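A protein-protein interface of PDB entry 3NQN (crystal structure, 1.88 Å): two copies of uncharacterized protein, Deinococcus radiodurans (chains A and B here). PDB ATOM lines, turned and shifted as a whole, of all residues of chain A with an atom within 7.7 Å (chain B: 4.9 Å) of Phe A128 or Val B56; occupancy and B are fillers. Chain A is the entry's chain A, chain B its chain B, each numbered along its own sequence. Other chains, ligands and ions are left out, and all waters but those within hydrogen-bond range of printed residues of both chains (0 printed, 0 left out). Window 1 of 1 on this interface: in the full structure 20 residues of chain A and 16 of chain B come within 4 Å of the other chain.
Hydrophobic or aromatic side chains of chain B within 4 Å of the printed part of chain A: Val B56, Leu B58, Leu B59, Phe B128, Met B131 and Val B132.
Along chain B the printed residues that touch a printed residue of chain A span positions 56 to 132.
Hydrophobic or aromatic side chains of chain A within 4 Å of the printed part of chain B: Val A56, Pro A57, Leu A58, Leu A59, Val A62, Ala A89, Ala A116, Ala A127, Phe A128, Met A131 and Val A132.
Among the printed residues, 22 pairs touch across the chains.
Of the printed residues of chain B, Phe A128 touches Val B56, Pro B57, Phe B128, Met B131 and Val B132.
Of chain A, only Phe A128 (3.6 Å) comes within 4 Å of Val B56.
Of chain A, only Phe A128 comes within 4 Å of Pro B57.
Of the printed residues of chain A, Met B131 touches Gly A124 (3.0 Å), Gly A125 (3.1 Å) and Phe A128 (3.4 Å).
Printed residues of chain B within 4 Å of Glu A87: Gly B60.
Printed residues of chain B within 4 Å of Glu A129: Leu B58.
Gln A133 touches none of the printed residues of chain B.
Thr B55 touches none of the printed residues of chain A.
The nearest printed residue of chain B that does not touch Phe A128 is Leu B59 (4.8 Å).
Pro A57 touches Phe B128, and with the chains exchanged Phe A128 touches Pro B57.
Val A62 touches Leu B59, but with the chains exchanged Leu A59 does not touch Val B62 (4.3 Å).
Phe A128 touches its own counterpart, Phe B128.
Phe A128 touches Met B131, and with the chains exchanged Met A131 touches Phe B128.
Of the 22 pairs that touch across the chains among the printed residues, 11 have their exchanged pair printed and touching as well.
The side-chain amide nitrogen (NE2) of Gln A133 lies within hydrogen-bond range of the side-chain carboxylate (OE2) of Glu A129 (3.2 Å).
N of Ala A89 sits at hydrogen-bond distance from O of Leu B59 (3.0 Å).
O of Leu B58 sits at hydrogen-bond distance from N of Ala A116, at 2.6 Å.
Among the printed residues, pairs that only touch across the chains: Val A56 with Phe B128 (3.98 Å), Pro A57 with Phe B128 (3.2 Å), Leu A58 with Val B132 (3.7 Å), Leu A59 with Val B132 (3.9 Å), Val A62 with Leu B59 (3.99 Å), Glu A87 with Gly B60 (3.5 Å), Arg A88 with Leu B59 (3.3 Å), Ala A89 with Leu B58 (3.7 Å), Gly A124 with Met B131 (3.0 Å), Gly A125 with Met B131 (3.1 Å), Ala A127 with Phe B128 (3.8 Å), Phe A128 with Val B56 (3.6 Å), Phe A128 with Pro B57 (3.4 Å), Phe A128 with Phe B128 (3.2 Å), Phe A128 with Met B131 (3.4 Å), Phe A128 with Val B132 (3.4 Å), Glu A129 with Leu B58 (3.7 Å), Met A131 with Phe B128 (3.5 Å), Val A132 with Leu B58 (3.9 Å) and Val A132 with Leu B59 (3.95 Å).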
ATOM      1  N   VAL A  56      -1.777  10.961  -4.834  1.00  0.00           N
ATOM      2  CA  VAL A  56      -0.903  10.218  -3.956  1.00  0.00           C
ATOM      3  C   VAL A  56      -0.138   9.214  -4.774  1.00  0.00           C
ATOM      4  O   VAL A  56      -0.533   8.895  -5.910  1.00  0.00           O
ATOM      5  CB  VAL A  56      -1.676   9.508  -2.802  1.00  0.00           C
ATOM      6  CG1 VAL A  56      -2.410  10.532  -1.951  1.00  0.00           C
ATOM      7  CG2 VAL A  56      -2.655   8.450  -3.353  1.00  0.00           C
ATOM      8  N   PRO A  57       0.967   8.701  -4.217  1.00  0.00           N
ATOM      9  CA  PRO A  57       1.735   7.729  -4.971  1.00  0.00           C
ATOM     10  C   PRO A  57       0.962   6.449  -5.274  1.00  0.00           C
ATOM     11  O   PRO A  57       0.149   5.987  -4.464  1.00  0.00           O
ATOM     12  CB  PRO A  57       2.936   7.424  -4.046  1.00  0.00           C
ATOM     13  CG  PRO A  57       3.069   8.639  -3.185  1.00  0.00           C
ATOM     14  CD  PRO A  57       1.676   9.148  -2.990  1.00  0.00           C
ATOM     15  N   LEU A  58       1.227   5.904  -6.443  1.00  0.00           N
ATOM     16  CA  LEU A  58       0.707   4.618  -6.868  1.00  0.00           C
ATOM     17  C   LEU A  58      -0.765   4.643  -7.265  1.00  0.00           C
ATOM     18  O   LEU A  58      -1.127   4.118  -8.315  1.00  0.00           O
ATOM     19  CB  LEU A  58       1.011   3.522  -5.828  1.00  0.00           C
ATOM     20  CG  LEU A  58       2.509   3.240  -5.552  1.00  0.00           C
ATOM     21  CD1 LEU A  58       2.646   1.993  -4.758  1.00  0.00           C
ATOM     22  CD2 LEU A  58       3.316   3.121  -6.839  1.00  0.00           C
ATOM     23  N   LEU A  59      -1.622   5.240  -6.445  1.00  0.00           N
ATOM     24  CA  LEU A  59      -3.028   5.419  -6.848  1.00  0.00           C
ATOM     25  C   LEU A  59      -3.163   6.545  -7.862  1.00  0.00           C
ATOM     26  O   LEU A  59      -4.066   6.530  -8.687  1.00  0.00           O
ATOM     27  CB  LEU A  59      -3.928   5.685  -5.641  1.00  0.00           C
ATOM     28  CG  LEU A  59      -4.012   4.537  -4.638  1.00  0.00           C
ATOM     29  CD1 LEU A  59      -4.817   4.986  -3.434  1.00  0.00           C
ATOM     30  CD2 LEU A  59      -4.616   3.277  -5.292  1.00  0.00           C
ATOM     31  N   VAL A  62      -6.713  10.752  -7.162  1.00  0.00           N
ATOM     32  CA  VAL A  62      -7.908  10.224  -6.520  1.00  0.00           C
ATOM     33  C   VAL A  62      -8.921  11.342  -6.431  1.00  0.00           C
ATOM     34  O   VAL A  62      -8.628  12.412  -5.894  1.00  0.00           O
ATOM     35  CB  VAL A  62      -7.605   9.683  -5.101  1.00  0.00           C
ATOM     36  CG1 VAL A  62      -8.918   9.147  -4.422  1.00  0.00           C
ATOM     37  CG2 VAL A  62      -6.533   8.567  -5.180  1.00  0.00           C
ATOM     38  N   GLU A  87     -18.026   6.238   2.829  1.00  0.00           N
ATOM     39  CA  GLU A  87     -17.369   5.127   2.100  1.00  0.00           C
ATOM     40  C   GLU A  87     -16.084   5.577   1.411  1.00  0.00           C
ATOM     41  O   GLU A  87     -15.179   4.775   1.166  1.00  0.00           O
ATOM     42  CB  GLU A  87     -18.324   4.551   1.060  1.00  0.00           C
ATOM     43  CG  GLU A  87     -18.534   5.461  -0.119  1.00  0.00           C
ATOM     44  CD  GLU A  87     -19.829   5.217  -0.810  1.00  0.00           C
ATOM     45  OE1 GLU A  87     -20.250   4.038  -0.896  1.00  0.00           O
ATOM     46  OE2 GLU A  87     -20.438   6.207  -1.264  1.00  0.00           O
ATOM     47  N   ARG A  88     -16.031   6.850   1.041  1.00  0.00           N
ATOM     48  CA  ARG A  88     -14.838   7.395   0.442  1.00  0.00           C
ATOM     49  C   ARG A  88     -14.709   8.836   0.801  1.00  0.00           C
ATOM     50  O   ARG A  88     -15.681   9.471   1.126  1.00  0.00           O
ATOM     51  CB  ARG A  88     -14.825   7.202  -1.072  1.00  0.00           C
ATOM     52  CG  ARG A  88     -15.969   7.826  -1.801  1.00  0.00           C
ATOM     53  CD  ARG A  88     -15.690   7.858  -3.304  1.00  0.00           C
ATOM     54  NE  ARG A  88     -16.822   8.402  -4.054  1.00  0.00           N
ATOM     55  CZ  ARG A  88     -16.738   8.918  -5.283  1.00  0.00           C
ATOM     56  NH1 ARG A  88     -15.566   9.007  -5.910  1.00  0.00           N
ATOM     57  NH2 ARG A  88     -17.823   9.378  -5.871  1.00  0.00           N
ATOM     58  N   ALA A  89     -13.478   9.335   0.767  1.00  0.00           N
ATOM     59  CA  ALA A  89     -13.179  10.726   1.082  1.00  0.00           C
ATOM     60  C   ALA A  89     -13.960  11.671   0.178  1.00  0.00           C
ATOM     61  O   ALA A  89     -14.219  11.363  -0.979  1.00  0.00           O
ATOM     62  CB  ALA A  89     -11.698  10.983   0.956  1.00  0.00           C
ATOM     63  N   ALA A 116     -12.241   9.210   5.228  1.00  0.00           N
ATOM     64  CA  ALA A 116     -12.945   7.990   5.625  1.00  0.00           C
ATOM     65  C   ALA A 116     -12.104   7.208   6.626  1.00  0.00           C
ATOM     66  O   ALA A 116     -12.629   6.399   7.385  1.00  0.00           O
ATOM     67  CB  ALA A 116     -13.240   7.129   4.380  1.00  0.00           C
ATOM     68  N   GLY A 122       0.169   0.474  12.921  1.00  0.00           N
ATOM     69  CA  GLY A 122       1.467   0.046  12.390  1.00  0.00           C
ATOM     70  C   GLY A 122       2.177   1.060  11.483  1.00  0.00           C
ATOM     71  O   GLY A 122       1.648   2.147  11.187  1.00  0.00           O
ATOM     72  N   TRP A 123       3.395   0.692  11.068  1.00  0.00           N
ATOM     73  CA  TRP A 123       4.225   1.486  10.142  1.00  0.00           C
ATOM     74  C   TRP A 123       3.424   1.782   8.851  1.00  0.00           C
ATOM     75  O   TRP A 123       3.297   2.932   8.441  1.00  0.00           O
ATOM     76  CB  TRP A 123       5.510   0.679   9.789  1.00  0.00           C
ATOM     77  CG  TRP A 123       6.587   1.440   9.016  1.00  0.00           C
ATOM     78  CD1 TRP A 123       6.501   2.696   8.503  1.00  0.00           C
ATOM     79  CD2 TRP A 123       7.864   0.925   8.593  1.00  0.00           C
ATOM     80  NE1 TRP A 123       7.654   3.018   7.829  1.00  0.00           N
ATOM     81  CE2 TRP A 123       8.507   1.949   7.867  1.00  0.00           C
ATOM     82  CE3 TRP A 123       8.542  -0.286   8.794  1.00  0.00           C
ATOM     83  CZ2 TRP A 123       9.795   1.801   7.340  1.00  0.00           C
ATOM     84  CZ3 TRP A 123       9.824  -0.432   8.263  1.00  0.00           C
ATOM     85  CH2 TRP A 123      10.434   0.609   7.551  1.00  0.00           C
ATOM     86  N   GLY A 124       2.895   0.729   8.219  1.00  0.00           N
ATOM     87  CA  GLY A 124       2.087   0.887   6.994  1.00  0.00           C
ATOM     88  C   GLY A 124       0.995   1.955   7.139  1.00  0.00           C
ATOM     89  O   GLY A 124       0.845   2.833   6.272  1.00  0.00           O
ATOM     90  N   GLY A 125       0.244   1.889   8.249  1.00  0.00           N
ATOM     91  CA  GLY A 125      -0.854   2.846   8.529  1.00  0.00           C
ATOM     92  C   GLY A 125      -0.398   4.262   8.852  1.00  0.00           C
ATOM     93  O   GLY A 125      -1.100   5.247   8.539  1.00  0.00           O
ATOM     94  N   ALA A 126       0.760   4.383   9.501  1.00  0.00           N
ATOM     95  CA  ALA A 126       1.308   5.703   9.847  1.00  0.00           C
ATOM     96  C   ALA A 126       1.795   6.421   8.580  1.00  0.00           C
ATOM     97  O   ALA A 126       1.527   7.611   8.392  1.00  0.00           O
ATOM     98  CB  ALA A 126       2.445   5.564  10.857  1.00  0.00           C
ATOM     99  N   ALA A 127       2.500   5.676   7.715  1.00  0.00           N
ATOM    100  CA  ALA A 127       2.999   6.209   6.435  1.00  0.00           C
ATOM    101  C   ALA A 127       1.841   6.636   5.528  1.00  0.00           C
ATOM    102  O   ALA A 127       1.913   7.671   4.855  1.00  0.00           O
ATOM    103  CB  ALA A 127       3.864   5.171   5.727  1.00  0.00           C
ATOM    104  N   PHE A 128       0.766   5.850   5.529  1.00  0.00           N
ATOM    105  CA  PHE A 128      -0.392   6.160   4.699  1.00  0.00           C
ATOM    106  C   PHE A 128      -1.101   7.434   5.162  1.00  0.00           C
ATOM    107  O   PHE A 128      -1.438   8.295   4.343  1.00  0.00           O
ATOM    108  CB  PHE A 128      -1.373   4.987   4.664  1.00  0.00           C
ATOM    109  CG  PHE A 128      -2.044   4.830   3.352  1.00  0.00           C
ATOM    110  CD1 PHE A 128      -1.426   4.131   2.338  1.00  0.00           C
ATOM    111  CD2 PHE A 128      -3.252   5.453   3.093  1.00  0.00           C
ATOM    112  CE1 PHE A 128      -2.021   4.015   1.099  1.00  0.00           C
ATOM    113  CE2 PHE A 128      -3.850   5.348   1.852  1.00  0.00           C
ATOM    114  CZ  PHE A 128      -3.239   4.630   0.857  1.00  0.00           C
ATOM    115  N   GLU A 129      -1.295   7.569   6.473  1.00  0.00           N
ATOM    116  CA  GLU A 129      -1.975   8.746   7.042  1.00  0.00           C
ATOM    117  C   GLU A 129      -1.208  10.032   6.756  1.00  0.00           C
ATOM    118  O   GLU A 129      -1.789  11.034   6.313  1.00  0.00           O
ATOM    119  CB  GLU A 129      -2.156   8.582   8.554  1.00  0.00           C
ATOM    120  CG  GLU A 129      -2.913   9.734   9.229  1.00  0.00           C
ATOM    121  CD  GLU A 129      -3.236   9.449  10.693  1.00  0.00           C
ATOM    122  OE1 GLU A 129      -2.437   8.742  11.357  1.00  0.00           O
ATOM    123  OE2 GLU A 129      -4.285   9.942  11.180  1.00  0.00           O
ATOM    124  N   LYS A 130       0.094  10.002   7.022  1.00  0.00           N
ATOM    125  CA  LYS A 130       0.963  11.158   6.792  1.00  0.00           C
ATOM    126  C   LYS A 130       0.857  11.653   5.356  1.00  0.00           C
ATOM    127  O   LYS A 130       0.635  12.833   5.117  1.00  0.00           O
ATOM    128  CB  LYS A 130       2.429  10.772   7.093  1.00  0.00           C
ATOM    129  CG  LYS A 130       3.457  11.904   6.875  1.00  0.00           C
ATOM    130  CD  LYS A 130       4.894  11.434   7.171  1.00  0.00           C
ATOM    131  N   MET A 131       0.970  10.720   4.411  1.00  0.00           N
ATOM    132  CA  MET A 131       0.957  11.032   2.965  1.00  0.00           C
ATOM    133  C   MET A 131      -0.404  11.542   2.505  1.00  0.00           C
ATOM    134  O   MET A 131      -0.491  12.492   1.717  1.00  0.00           O
ATOM    135  CB  MET A 131       1.329   9.776   2.162  1.00  0.00           C
ATOM    136  CG  MET A 131       1.319   9.929   0.629  1.00  0.00           C
ATOM    137  SD  MET A 131       2.831  10.935  -0.121  1.00  0.00           S
ATOM    138  CE  MET A 131       2.042  12.688  -0.088  1.00  0.00           C
ATOM    139  N   VAL A 132      -1.480  10.910   2.988  1.00  0.00           N
ATOM    140  CA  VAL A 132      -2.840  11.325   2.571  1.00  0.00           C
ATOM    141  C   VAL A 132      -3.231  12.713   3.099  1.00  0.00           C
ATOM    142  O   VAL A 132      -3.810  13.506   2.356  1.00  0.00           O
ATOM    143  CB  VAL A 132      -3.939  10.298   2.952  1.00  0.00           C
ATOM    144  CG1 VAL A 132      -5.347  10.887   2.679  1.00  0.00           C
ATOM    145  CG2 VAL A 132      -3.744   8.986   2.186  1.00  0.00           C
ATOM    146  N   GLN A 133      -2.945  13.004   4.375  1.00  0.00           N
ATOM    147  CA  GLN A 133      -3.277  14.313   4.949  1.00  0.00           C
ATOM    148  C   GLN A 133      -2.536  15.445   4.235  1.00  0.00           C
ATOM    149  O   GLN A 133      -3.121  16.478   3.912  1.00  0.00           O
ATOM    150  CB  GLN A 133      -2.958  14.339   6.439  1.00  0.00           C
ATOM    151  CG  GLN A 133      -3.854  13.438   7.268  1.00  0.00           C
ATOM    152  CD  GLN A 133      -3.489  13.448   8.734  1.00  0.00           C
ATOM    153  OE1 GLN A 133      -2.522  14.089   9.141  1.00  0.00           O
ATOM    154  NE2 GLN A 133      -4.266  12.743   9.536  1.00  0.00           N
ATOM    155  N   ALA A 134      -1.248  15.236   3.987  1.00  0.00           N
ATOM    156  CA  ALA A 134      -0.424  16.235   3.304  1.00  0.00           C
ATOM    157  C   ALA A 134      -0.932  16.495   1.884  1.00  0.00           C
ATOM    158  O   ALA A 134      -1.024  17.637   1.443  1.00  0.00           O
ATOM    159  CB  ALA A 134       1.044  15.778   3.271  1.00  0.00           C
ATOM    160  N   VAL B  54     -10.626  -0.653  -4.546  1.00  0.00           N
ATOM    161  CA  VAL B  54      -9.517  -0.885  -3.640  1.00  0.00           C
ATOM    162  C   VAL B  54      -9.754  -0.023  -2.395  1.00  0.00           C
ATOM    163  O   VAL B  54      -9.909   1.205  -2.500  1.00  0.00           O
ATOM    164  CB  VAL B  54      -8.183  -0.523  -4.296  1.00  0.00           C
ATOM    165  CG1 VAL B  54      -7.055  -0.644  -3.316  1.00  0.00           C
ATOM    166  CG2 VAL B  54      -7.927  -1.430  -5.548  1.00  0.00           C
ATOM    167  N   THR B  55      -9.839  -0.663  -1.225  1.00  0.00           N
ATOM    168  CA  THR B  55     -10.081   0.067   0.026  1.00  0.00           C
ATOM    169  C   THR B  55      -8.802   0.374   0.777  1.00  0.00           C
ATOM    170  O   THR B  55      -8.061  -0.531   1.145  1.00  0.00           O
ATOM    171  CB  THR B  55     -11.028  -0.694   0.953  1.00  0.00           C
ATOM    172  OG1 THR B  55     -12.294  -0.837   0.312  1.00  0.00           O
ATOM    173  CG2 THR B  55     -11.222   0.067   2.257  1.00  0.00           C
ATOM    174  N   VAL B  56      -8.547   1.666   1.012  1.00  0.00           N
ATOM    175  CA  VAL B  56      -7.378   2.083   1.765  1.00  0.00           C
ATOM    176  C   VAL B  56      -7.767   3.042   2.860  1.00  0.00           C
ATOM    177  O   VAL B  56      -8.839   3.623   2.816  1.00  0.00           O
ATOM    178  CB  VAL B  56      -6.291   2.724   0.848  1.00  0.00           C
ATOM    179  CG1 VAL B  56      -5.889   1.730  -0.251  1.00  0.00           C
ATOM    180  CG2 VAL B  56      -6.777   4.036   0.243  1.00  0.00           C
ATOM    181  N   PRO B  57      -6.923   3.153   3.897  1.00  0.00           N
ATOM    182  CA  PRO B  57      -7.172   4.090   4.978  1.00  0.00           C
ATOM    183  C   PRO B  57      -7.398   5.525   4.472  1.00  0.00           C
ATOM    184  O   PRO B  57      -6.747   5.959   3.503  1.00  0.00           O
ATOM    185  CB  PRO B  57      -5.871   4.041   5.794  1.00  0.00           C
ATOM    186  CG  PRO B  57      -5.293   2.695   5.506  1.00  0.00           C
ATOM    187  CD  PRO B  57      -5.693   2.365   4.109  1.00  0.00           C
ATOM    188  N   LEU B  58      -8.314   6.226   5.132  1.00  0.00           N
ATOM    189  CA  LEU B  58      -8.578   7.676   4.903  1.00  0.00           C
ATOM    190  C   LEU B  58      -9.278   7.997   3.579  1.00  0.00           C
ATOM    191  O   LEU B  58     -10.274   8.719   3.575  1.00  0.00           O
ATOM    192  CB  LEU B  58      -7.308   8.511   5.074  1.00  0.00           C
ATOM    193  CG  LEU B  58      -6.541   8.303   6.403  1.00  0.00           C
ATOM    194  CD1 LEU B  58      -5.587   9.453   6.629  1.00  0.00           C
ATOM    195  CD2 LEU B  58      -7.487   8.150   7.605  1.00  0.00           C
ATOM    196  N   LEU B  59      -8.770   7.473   2.466  1.00  0.00           N
ATOM    197  CA  LEU B  59      -9.436   7.681   1.164  1.00  0.00           C
ATOM    198  C   LEU B  59     -10.628   6.749   1.011  1.00  0.00           C
ATOM    199  O   LEU B  59     -11.554   7.057   0.293  1.00  0.00           O
ATOM    200  CB  LEU B  59      -8.474   7.478   0.011  1.00  0.00           C
ATOM    201  CG  LEU B  59      -7.290   8.430  -0.091  1.00  0.00           C
ATOM    202  CD1 LEU B  59      -6.399   8.013  -1.229  1.00  0.00           C
ATOM    203  CD2 LEU B  59      -7.764   9.862  -0.276  1.00  0.00           C
ATOM    204  N   GLY B  60     -10.600   5.606   1.708  1.00  0.00           N
ATOM    205  CA  GLY B  60     -11.690   4.640   1.638  1.00  0.00           C
ATOM    206  C   GLY B  60     -11.681   3.864   0.328  1.00  0.00           C
ATOM    207  O   GLY B  60     -10.626   3.412  -0.134  1.00  0.00           O
ATOM    208  N   VAL B  62     -11.485   3.263  -3.388  1.00  0.00           N
ATOM    209  CA  VAL B  62     -10.892   3.868  -4.556  1.00  0.00           C
ATOM    210  C   VAL B  62     -11.149   2.974  -5.762  1.00  0.00           C
ATOM    211  O   VAL B  62     -10.737   1.811  -5.794  1.00  0.00           O
ATOM    212  CB  VAL B  62      -9.378   4.053  -4.372  1.00  0.00           C
ATOM    213  CG1 VAL B  62      -8.750   4.708  -5.628  1.00  0.00           C
ATOM    214  CG2 VAL B  62      -9.101   4.879  -3.117  1.00  0.00           C
ATOM    215  N   PHE B 128       4.561   3.383   2.267  1.00  0.00           N
ATOM    216  CA  PHE B 128       3.337   3.775   1.589  1.00  0.00           C
ATOM    217  C   PHE B 128       3.038   2.860   0.406  1.00  0.00           C
ATOM    218  O   PHE B 128       1.911   2.442   0.229  1.00  0.00           O
ATOM    219  CB  PHE B 128       3.408   5.220   1.092  1.00  0.00           C
ATOM    220  CG  PHE B 128       2.097   5.732   0.560  1.00  0.00           C
ATOM    221  CD1 PHE B 128       1.158   6.280   1.416  1.00  0.00           C
ATOM    222  CD2 PHE B 128       1.782   5.621  -0.792  1.00  0.00           C
ATOM    223  CE1 PHE B 128      -0.070   6.723   0.941  1.00  0.00           C
ATOM    224  CE2 PHE B 128       0.554   6.065  -1.273  1.00  0.00           C
ATOM    225  CZ  PHE B 128      -0.371   6.610  -0.407  1.00  0.00           C
ATOM    226  N   MET B 131       1.597  -0.658   1.326  1.00  0.00           N
ATOM    227  CA  MET B 131       0.190  -0.605   1.736  1.00  0.00           C
ATOM    228  C   MET B 131      -0.724  -0.588   0.517  1.00  0.00           C
ATOM    229  O   MET B 131      -1.715  -1.320   0.467  1.00  0.00           O
ATOM    230  CB  MET B 131      -0.084   0.642   2.580  1.00  0.00           C
ATOM    231  CG  MET B 131      -1.572   0.838   2.946  1.00  0.00           C
ATOM    232  SD  MET B 131      -2.132  -0.215   4.488  1.00  0.00           S
ATOM    233  CE  MET B 131      -1.536   0.988   5.882  1.00  0.00           C
ATOM    234  N   VAL B 132      -0.413   0.282  -0.444  1.00  0.00           N
ATOM    235  CA  VAL B 132      -1.209   0.385  -1.663  1.00  0.00           C
ATOM    236  C   VAL B 132      -1.172  -0.944  -2.418  1.00  0.00           C
ATOM    237  O   VAL B 132      -2.198  -1.420  -2.915  1.00  0.00           O
ATOM    238  CB  VAL B 132      -0.692   1.507  -2.592  1.00  0.00           C
ATOM    239  CG1 VAL B 132      -1.466   1.498  -3.942  1.00  0.00           C
ATOM    240  CG2 VAL B 132      -0.822   2.855  -1.915  1.00  0.00           C
ATOM    241  N   ALA B 135      -3.279  -3.587  -0.660  1.00  0.00           N
ATOM    242  CA  ALA B 135      -4.709  -3.330  -0.862  1.00  0.00           C
ATOM    243  C   ALA B 135      -5.130  -3.705  -2.280  1.00  0.00           C
ATOM    244  O   ALA B 135      -6.190  -4.314  -2.498  1.00  0.00           O
ATOM    245  CB  ALA B 135      -5.024  -1.851  -0.585  1.00  0.00           C
